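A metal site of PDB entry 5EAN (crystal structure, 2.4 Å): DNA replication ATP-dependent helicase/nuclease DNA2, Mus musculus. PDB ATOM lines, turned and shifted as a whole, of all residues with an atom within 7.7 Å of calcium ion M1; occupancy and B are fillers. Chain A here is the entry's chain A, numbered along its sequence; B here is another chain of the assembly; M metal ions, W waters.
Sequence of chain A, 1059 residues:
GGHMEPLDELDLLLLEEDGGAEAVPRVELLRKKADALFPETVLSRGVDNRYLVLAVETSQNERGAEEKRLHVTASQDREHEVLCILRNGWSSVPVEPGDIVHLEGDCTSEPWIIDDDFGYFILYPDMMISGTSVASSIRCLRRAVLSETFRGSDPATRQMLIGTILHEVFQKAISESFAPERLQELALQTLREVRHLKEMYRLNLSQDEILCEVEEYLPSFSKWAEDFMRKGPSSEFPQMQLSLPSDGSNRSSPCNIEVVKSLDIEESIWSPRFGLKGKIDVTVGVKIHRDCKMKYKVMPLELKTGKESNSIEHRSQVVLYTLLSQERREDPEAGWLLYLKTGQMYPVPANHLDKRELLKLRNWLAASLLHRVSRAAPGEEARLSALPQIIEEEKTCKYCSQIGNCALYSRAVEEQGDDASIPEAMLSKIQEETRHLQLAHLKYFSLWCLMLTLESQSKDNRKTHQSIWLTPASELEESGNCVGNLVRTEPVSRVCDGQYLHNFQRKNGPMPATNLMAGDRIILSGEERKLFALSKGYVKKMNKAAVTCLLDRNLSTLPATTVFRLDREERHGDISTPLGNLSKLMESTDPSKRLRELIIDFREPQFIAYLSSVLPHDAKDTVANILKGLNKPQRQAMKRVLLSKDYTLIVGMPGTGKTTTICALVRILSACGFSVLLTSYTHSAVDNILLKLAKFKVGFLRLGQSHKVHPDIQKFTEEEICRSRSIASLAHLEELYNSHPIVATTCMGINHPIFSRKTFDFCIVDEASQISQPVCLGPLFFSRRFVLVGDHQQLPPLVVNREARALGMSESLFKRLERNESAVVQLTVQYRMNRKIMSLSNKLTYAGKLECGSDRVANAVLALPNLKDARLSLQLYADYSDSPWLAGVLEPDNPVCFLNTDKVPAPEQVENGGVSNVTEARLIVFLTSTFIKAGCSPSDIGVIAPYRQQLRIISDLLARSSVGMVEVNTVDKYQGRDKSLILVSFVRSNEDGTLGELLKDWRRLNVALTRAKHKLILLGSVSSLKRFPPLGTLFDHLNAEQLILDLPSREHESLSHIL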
ATOM      1  N   GLY A 163       4.049  16.887  14.288  1.00  0.00           N
ATOM      2  CA  GLY A 163       5.477  16.779  14.032  1.00  0.00           C
ATOM      3  C   GLY A 163       6.322  16.527  15.252  1.00  0.00           C
ATOM      4  O   GLY A 163       7.150  15.633  15.245  1.00  0.00           O
ATOM      5  N   HIS A 167       8.335  12.953  15.955  1.00  0.00           N
ATOM      6  CA  HIS A 167       9.768  13.011  16.236  1.00  0.00           C
ATOM      7  C   HIS A 167      10.063  12.162  17.481  1.00  0.00           C
ATOM      8  O   HIS A 167      10.875  11.235  17.428  1.00  0.00           O
ATOM      9  CB  HIS A 167      10.236  14.472  16.440  1.00  0.00           C
ATOM     10  CG  HIS A 167      10.633  15.207  15.187  1.00  0.00           C
ATOM     11  ND1 HIS A 167       9.732  15.559  14.206  1.00  0.00           N
ATOM     12  CD2 HIS A 167      11.825  15.731  14.800  1.00  0.00           C
ATOM     13  CE1 HIS A 167      10.360  16.241  13.252  1.00  0.00           C
ATOM     14  NE2 HIS A 167      11.630  16.353  13.584  1.00  0.00           N
ATOM     15  N   GLN A 171      12.092   8.603  17.869  1.00  0.00           N
ATOM     16  CA  GLN A 171      13.286   8.607  18.669  1.00  0.00           C
ATOM     17  C   GLN A 171      13.200   7.567  19.776  1.00  0.00           C
ATOM     18  O   GLN A 171      14.205   6.981  20.118  1.00  0.00           O
ATOM     19  CB  GLN A 171      13.554   9.999  19.217  1.00  0.00           C
ATOM     20  CG  GLN A 171      14.072  10.956  18.145  1.00  0.00           C
ATOM     21  CD  GLN A 171      14.039  12.414  18.586  1.00  0.00           C
ATOM     22  OE1 GLN A 171      13.327  12.790  19.532  1.00  0.00           O
ATOM     23  NE2 GLN A 171      14.845  13.246  17.910  1.00  0.00           N
ATOM     24  N   GLU A 266      18.718  13.850  19.658  1.00  0.00           N
ATOM     25  CA  GLU A 266      18.582  15.250  20.046  1.00  0.00           C
ATOM     26  C   GLU A 266      19.910  15.886  20.434  1.00  0.00           C
ATOM     27  O   GLU A 266      20.036  16.501  21.488  1.00  0.00           O
ATOM     28  CB  GLU A 266      17.557  15.380  21.204  1.00  0.00           C
ATOM     29  CG  GLU A 266      16.119  15.129  20.805  1.00  0.00           C
ATOM     30  CD  GLU A 266      15.557  16.255  19.946  1.00  0.00           C
ATOM     31  OE1 GLU A 266      15.545  16.127  18.691  1.00  0.00           O
ATOM     32  OE2 GLU A 266      15.157  17.291  20.548  1.00  0.00           O
ATOM     33  N   LYS A 279      20.352  21.283  16.477  1.00  0.00           N
ATOM     34  CA  LYS A 279      19.970  20.054  17.155  1.00  0.00           C
ATOM     35  C   LYS A 279      19.819  18.989  16.065  1.00  0.00           C
ATOM     36  O   LYS A 279      19.004  19.150  15.167  1.00  0.00           O
ATOM     37  CB  LYS A 279      18.671  20.280  17.929  1.00  0.00           C
ATOM     38  CG  LYS A 279      18.464  19.356  19.103  1.00  0.00           C
ATOM     39  CD  LYS A 279      17.298  19.804  19.996  1.00  0.00           C
ATOM     40  CE  LYS A 279      17.624  19.565  21.479  1.00  0.00           C
ATOM     41  NZ  LYS A 279      16.556  18.912  22.321  1.00  0.00           N
ATOM     42  N   ILE A 280      20.637  17.938  16.126  1.00  0.00           N
ATOM     43  CA  ILE A 280      20.487  16.775  15.224  1.00  0.00           C
ATOM     44  C   ILE A 280      19.420  15.848  15.821  1.00  0.00           C
ATOM     45  O   ILE A 280      19.567  15.397  16.960  1.00  0.00           O
ATOM     46  CB  ILE A 280      21.838  16.047  14.970  1.00  0.00           C
ATOM     47  CG1 ILE A 280      22.824  16.967  14.235  1.00  0.00           C
ATOM     48  CG2 ILE A 280      21.627  14.782  14.132  1.00  0.00           C
ATOM     49  CD1 ILE A 280      24.286  16.583  14.380  1.00  0.00           C
ATOM     50  N   ASP A 281      18.371  15.589  15.043  1.00  0.00           N
ATOM     51  CA  ASP A 281      17.274  14.711  15.451  1.00  0.00           C
ATOM     52  C   ASP A 281      17.814  13.340  15.892  1.00  0.00           C
ATOM     53  O   ASP A 281      17.511  12.873  17.009  1.00  0.00           O
ATOM     54  CB  ASP A 281      16.271  14.511  14.313  1.00  0.00           C
ATOM     55  CG  ASP A 281      15.382  15.716  14.091  1.00  0.00           C
ATOM     56  OD1 ASP A 281      15.127  16.463  15.045  1.00  0.00           O
ATOM     57  OD2 ASP A 281      14.933  15.918  12.949  1.00  0.00           O
ATOM     58  N   VAL A 282      18.588  12.702  15.001  1.00  0.00           N
ATOM     59  CA  VAL A 282      19.172  11.394  15.266  1.00  0.00           C
ATOM     60  C   VAL A 282      20.541  11.335  14.615  1.00  0.00           C
ATOM     61  O   VAL A 282      20.725  11.651  13.441  1.00  0.00           O
ATOM     62  CB  VAL A 282      18.369  10.188  14.691  1.00  0.00           C
ATOM     63  CG1 VAL A 282      18.614   8.946  15.523  1.00  0.00           C
ATOM     64  CG2 VAL A 282      16.873  10.452  14.615  1.00  0.00           C
ATOM     65  N   LEU A 301      20.860  12.548  10.896  1.00  0.00           N
ATOM     66  CA  LEU A 301      19.587  12.242  10.231  1.00  0.00           C
ATOM     67  C   LEU A 301      18.549  13.286  10.644  1.00  0.00           C
ATOM     68  O   LEU A 301      18.343  13.552  11.847  1.00  0.00           O
ATOM     69  CB  LEU A 301      19.120  10.816  10.567  1.00  0.00           C
ATOM     70  CG  LEU A 301      17.655  10.427  10.252  1.00  0.00           C
ATOM     71  CD1 LEU A 301      17.333  10.528   8.759  1.00  0.00           C
ATOM     72  CD2 LEU A 301      17.335   9.035  10.764  1.00  0.00           C
ATOM     73  N   GLU A 302      17.888  13.880   9.657  1.00  0.00           N
ATOM     74  CA  GLU A 302      16.889  14.906   9.905  1.00  0.00           C
ATOM     75  C   GLU A 302      15.497  14.318   9.670  1.00  0.00           C
ATOM     76  O   GLU A 302      15.234  13.786   8.583  1.00  0.00           O
ATOM     77  CB  GLU A 302      17.160  16.126   9.000  1.00  0.00           C
ATOM     78  CG  GLU A 302      16.143  17.260   9.041  1.00  0.00           C
ATOM     79  CD  GLU A 302      15.862  17.841  10.424  1.00  0.00           C
ATOM     80  OE1 GLU A 302      14.700  18.168  10.690  1.00  0.00           O
ATOM     81  OE2 GLU A 302      16.807  17.981  11.245  1.00  0.00           O
ATOM     82  N   LEU A 303      14.622  14.423  10.659  1.00  0.00           N
ATOM     83  CA  LEU A 303      13.240  13.945  10.500  1.00  0.00           C
ATOM     84  C   LEU A 303      12.278  15.077  10.114  1.00  0.00           C
ATOM     85  O   LEU A 303      12.357  16.166  10.659  1.00  0.00           O
ATOM     86  CB  LEU A 303      12.758  13.242  11.769  1.00  0.00           C
ATOM     87  CG  LEU A 303      13.712  12.297  12.484  1.00  0.00           C
ATOM     88  CD1 LEU A 303      13.073  11.949  13.812  1.00  0.00           C
ATOM     89  CD2 LEU A 303      14.010  11.035  11.678  1.00  0.00           C
ATOM     90  N   LYS A 304      11.388  14.791   9.167  1.00  0.00           N
ATOM     91  CA  LYS A 304      10.395  15.753   8.670  1.00  0.00           C
ATOM     92  C   LYS A 304       9.037  15.080   8.578  1.00  0.00           C
ATOM     93  O   LYS A 304       8.906  13.987   8.038  1.00  0.00           O
ATOM     94  CB  LYS A 304      10.759  16.257   7.272  1.00  0.00           C
ATOM     95  CG  LYS A 304      12.024  17.070   7.142  1.00  0.00           C
ATOM     96  CD  LYS A 304      11.845  18.467   7.719  1.00  0.00           C
ATOM     97  CE  LYS A 304      13.179  19.175   7.845  1.00  0.00           C
ATOM     98  NZ  LYS A 304      13.068  20.404   8.675  1.00  0.00           N
ATOM     99  N   THR A 305       8.023  15.725   9.129  1.00  0.00           N
ATOM    100  CA  THR A 305       6.671  15.240   9.001  1.00  0.00           C
ATOM    101  C   THR A 305       6.024  16.122   7.944  1.00  0.00           C
ATOM    102  O   THR A 305       6.663  17.050   7.463  1.00  0.00           O
ATOM    103  CB  THR A 305       5.948  15.257  10.356  1.00  0.00           C
ATOM    104  OG1 THR A 305       5.989  16.575  10.868  1.00  0.00           O
ATOM    105  CG2 THR A 305       6.650  14.345  11.353  1.00  0.00           C
ATOM    106  N   GLN A 317      19.563  22.610   5.594  1.00  0.00           N
ATOM    107  CA  GLN A 317      19.647  22.271   7.029  1.00  0.00           C
ATOM    108  C   GLN A 317      20.559  21.083   7.281  1.00  0.00           C
ATOM    109  O   GLN A 317      21.422  21.116   8.161  1.00  0.00           O
ATOM    110  CB  GLN A 317      18.300  21.961   7.636  1.00  0.00           C
ATOM    111  CG  GLN A 317      17.294  23.104   7.702  1.00  0.00           C
ATOM    112  CD  GLN A 317      15.862  22.598   7.937  1.00  0.00           C
ATOM    113  OE1 GLN A 317      15.646  21.544   8.566  1.00  0.00           O
ATOM    114  NE2 GLN A 317      14.879  23.341   7.410  1.00  0.00           N
ATOM    115  N   TYR A 321      24.091  20.703   9.266  1.00  0.00           N
ATOM    116  CA  TYR A 321      24.320  19.659  10.291  1.00  0.00           C
ATOM    117  C   TYR A 321      25.662  18.941  10.126  1.00  0.00           C
ATOM    118  O   TYR A 321      26.256  18.529  11.124  1.00  0.00           O
ATOM    119  CB  TYR A 321      23.162  18.655  10.388  1.00  0.00           C
ATOM    120  CG  TYR A 321      21.905  19.251  10.954  1.00  0.00           C
ATOM    121  CD1 TYR A 321      21.955  20.006  12.130  1.00  0.00           C
ATOM    122  CD2 TYR A 321      20.670  19.091  10.317  1.00  0.00           C
ATOM    123  CE1 TYR A 321      20.818  20.585  12.657  1.00  0.00           C
ATOM    124  CE2 TYR A 321      19.523  19.672  10.843  1.00  0.00           C
ATOM    125  CZ  TYR A 321      19.598  20.399  12.022  1.00  0.00           C
ATOM    126  OH  TYR A 321      18.483  20.991  12.587  1.00  0.00           O
ATOM    127  N   LEU A 337      17.803  12.975   5.055  1.00  0.00           N
ATOM    128  CA  LEU A 337      16.474  13.542   5.238  1.00  0.00           C
ATOM    129  C   LEU A 337      15.477  12.413   5.161  1.00  0.00           C
ATOM    130  O   LEU A 337      15.337  11.782   4.100  1.00  0.00           O
ATOM    131  CB  LEU A 337      16.119  14.455   4.078  1.00  0.00           C
ATOM    132  CG  LEU A 337      16.179  15.960   4.168  1.00  0.00           C
ATOM    133  CD1 LEU A 337      15.781  16.577   2.814  1.00  0.00           C
ATOM    134  CD2 LEU A 337      15.305  16.453   5.307  1.00  0.00           C
ATOM    135  N   LEU A 338      14.753  12.197   6.254  1.00  0.00           N
ATOM    136  CA  LEU A 338      13.684  11.229   6.243  1.00  0.00           C
ATOM    137  C   LEU A 338      12.322  11.944   6.373  1.00  0.00           C
ATOM    138  O   LEU A 338      12.067  12.693   7.350  1.00  0.00           O
ATOM    139  CB  LEU A 338      13.933  10.184   7.345  1.00  0.00           C
ATOM    140  CG  LEU A 338      12.857   9.202   7.812  1.00  0.00           C
ATOM    141  CD1 LEU A 338      12.320   8.403   6.642  1.00  0.00           C
ATOM    142  CD2 LEU A 338      13.436   8.289   8.895  1.00  0.00           C
ATOM    143  N   LEU A 340       8.949  11.221   7.309  1.00  0.00           N
ATOM    144  CA  LEU A 340       8.220  10.205   8.082  1.00  0.00           C
ATOM    145  C   LEU A 340       6.839   9.817   7.506  1.00  0.00           C
ATOM    146  O   LEU A 340       6.373   8.716   7.741  1.00  0.00           O
ATOM    147  CB  LEU A 340       8.117  10.604   9.560  1.00  0.00           C
ATOM    148  CG  LEU A 340       9.413  10.765  10.332  1.00  0.00           C
ATOM    149  CD1 LEU A 340       9.179  11.429  11.675  1.00  0.00           C
ATOM    150  CD2 LEU A 340      10.090   9.407  10.488  1.00  0.00           C
ATOM    151  P    DG B  11      18.200  23.754  14.908  1.00  0.00           P
ATOM    152  OP1  DG B  11      19.200  22.779  14.422  1.00  0.00           O
ATOM    153  OP2  DG B  11      18.082  25.083  14.238  1.00  0.00           O
ATOM    154  O5'  DG B  11      16.850  22.913  14.848  1.00  0.00           O
ATOM    155  C5'  DG B  11      15.637  23.471  15.381  1.00  0.00           C
ATOM    156  C4'  DG B  11      14.518  22.454  15.380  1.00  0.00           C
ATOM    157  O4'  DG B  11      13.471  22.990  16.220  1.00  0.00           O
ATOM    158  C3'  DG B  11      13.856  22.271  14.018  1.00  0.00           C
ATOM    159  O3'  DG B  11      12.971  21.139  13.895  1.00  0.00           O
ATOM    160  C2'  DG B  11      12.971  23.502  13.946  1.00  0.00           C
ATOM    161  C1'  DG B  11      12.488  23.611  15.399  1.00  0.00           C
ATOM    162  N9   DG B  11      12.272  24.968  15.904  1.00  0.00           N
ATOM    163  C8   DG B  11      12.794  26.140  15.410  1.00  0.00           C
ATOM    164  N7   DG B  11      12.416  27.190  16.074  1.00  0.00           N
ATOM    165  C5   DG B  11      11.587  26.680  17.077  1.00  0.00           C
ATOM    166  C6   DG B  11      10.869  27.352  18.104  1.00  0.00           C
ATOM    167  O6   DG B  11      10.831  28.561  18.352  1.00  0.00           O
ATOM    168  N1   DG B  11      10.151  26.449  18.889  1.00  0.00           N
ATOM    169  C2   DG B  11      10.130  25.093  18.709  1.00  0.00           C
ATOM    170  N2   DG B  11       9.377  24.392  19.580  1.00  0.00           N
ATOM    171  N3   DG B  11      10.782  24.458  17.755  1.00  0.00           N
ATOM    172  C4   DG B  11      11.491  25.308  16.970  1.00  0.00           C
ATOM    173  P    DA B  12      13.127  19.751  14.749  1.00  0.00           P
ATOM    174  OP1  DA B  12      13.628  20.053  16.111  1.00  0.00           O
ATOM    175  OP2  DA B  12      13.822  18.755  13.886  1.00  0.00           O
ATOM    176  O5'  DA B  12      11.598  19.322  14.973  1.00  0.00           O
ATOM    177  C5'  DA B  12      10.631  20.355  15.215  1.00  0.00           C
ATOM    178  C4'  DA B  12       9.212  19.843  15.104  1.00  0.00           C
ATOM    179  O4'  DA B  12       8.450  20.601  16.075  1.00  0.00           O
ATOM    180  C3'  DA B  12       8.541  20.096  13.748  1.00  0.00           C
ATOM    181  O3'  DA B  12       8.291  18.901  12.998  1.00  0.00           O
ATOM    182  C2'  DA B  12       7.198  20.708  14.098  1.00  0.00           C
ATOM    183  C1'  DA B  12       7.464  21.380  15.433  1.00  0.00           C
ATOM    184  N9   DA B  12       7.942  22.771  15.342  1.00  0.00           N
ATOM    185  C8   DA B  12       8.749  23.322  14.386  1.00  0.00           C
ATOM    186  N7   DA B  12       8.979  24.600  14.553  1.00  0.00           N
ATOM    187  C5   DA B  12       8.253  24.910  15.698  1.00  0.00           C
ATOM    188  C6   DA B  12       8.077  26.113  16.405  1.00  0.00           C
ATOM    189  N6   DA B  12       8.637  27.277  16.051  1.00  0.00           N
ATOM    190  N1   DA B  12       7.297  26.087  17.513  1.00  0.00           N
ATOM    191  C2   DA B  12       6.727  24.925  17.867  1.00  0.00           C
ATOM    192  N3   DA B  12       6.822  23.730  17.285  1.00  0.00           N
ATOM    193  C4   DA B  12       7.608  23.793  16.192  1.00  0.00           C
ATOM    194  P    DG B  13       8.319  18.910  11.381  1.00  0.00           P
ATOM    195  OP1  DG B  13       8.423  17.498  10.931  1.00  0.00           O
ATOM    196  OP2  DG B  13       9.351  19.871  10.934  1.00  0.00           O
ATOM    197  O5'  DG B  13       6.883  19.472  10.973  1.00  0.00           O
ATOM    198  C5'  DG B  13       6.494  19.493   9.573  1.00  0.00           C
ATOM    199  C4'  DG B  13       5.159  20.170   9.346  1.00  0.00           C
ATOM    200  O4'  DG B  13       5.015  21.334  10.192  1.00  0.00           O
ATOM    201  C3'  DG B  13       4.948  20.704   7.922  1.00  0.00           C
ATOM    202  O3'  DG B  13       3.555  20.745   7.618  1.00  0.00           O
ATOM    203  C2'  DG B  13       5.520  22.110   7.996  1.00  0.00           C
ATOM    204  C1'  DG B  13       5.268  22.526   9.447  1.00  0.00           C
ATOM    205  N9   DG B  13       6.388  23.205  10.070  1.00  0.00           N
ATOM    206  C8   DG B  13       7.589  22.635  10.445  1.00  0.00           C
ATOM    207  N7   DG B  13       8.405  23.478  11.020  1.00  0.00           N
ATOM    208  C5   DG B  13       7.705  24.673  11.036  1.00  0.00           C
ATOM    209  C6   DG B  13       8.074  25.949  11.526  1.00  0.00           C
ATOM    210  O6   DG B  13       9.141  26.288  12.068  1.00  0.00           O
ATOM    211  N1   DG B  13       7.064  26.892  11.332  1.00  0.00           N
ATOM    212  C2   DG B  13       5.850  26.631  10.744  1.00  0.00           C
ATOM    213  N2   DG B  13       5.001  27.676  10.657  1.00  0.00           N
ATOM    214  N3   DG B  13       5.488  25.448  10.290  1.00  0.00           N
ATOM    215  C4   DG B  13       6.451  24.522  10.465  1.00  0.00           C
HETATM  216 CA    CA M   1      13.281  17.427  12.350  1.00  0.00          CA
HETATM  217 CA    CA M   2      12.440  21.066  11.651  1.00  0.00          CA
HETATM  218  O   HOH W   1      11.927  18.942  11.543  1.00  0.00           O
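OE1 of Glu 302 sits close to NZ of Lys 304 (3.4 Å).
O of Glu 302 lies within hydrogen-bond range of N of Leu 338, at 2.9 Å.
The backbone NH (N) of Glu 266 sits at hydrogen-bond distance from the backbone carbonyl oxygen (O) of Asp 281, at 3.1 Å.
The backbone carbonyl oxygen of Asp 281 is in hydrogen-bond range of the side-chain amide nitrogen of Gln 171, at 2.8 Å.
A ring nitrogen (ND1) of His 167 lies within hydrogen-bond range of the backbone carbonyl oxygen of Gly 163 (2.8 Å).
Water W1 lies within hydrogen-bond range of OP2 of DG 13 of chain B, the side-chain amino group (NZ) of Lys 304 and O5' of DA 12 of chain B.
The nearest printed residue that does not touch calcium ion M1 is DG 11 of chain B (4.03 Å).
OP2 of DA 12 of chain B binds calcium ion M1 (2.1 Å).
Water W1 binds calcium ion M1 (2.2 Å).
O of Leu 303 binds calcium ion M1.
OE1 of Glu 302 binds calcium ion M1.
Calcium ion M1 is bound by OD2 of Asp 281 (2.3 Å).
NE2 of His 167 is bound to calcium ion M1 (2.3 Å).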
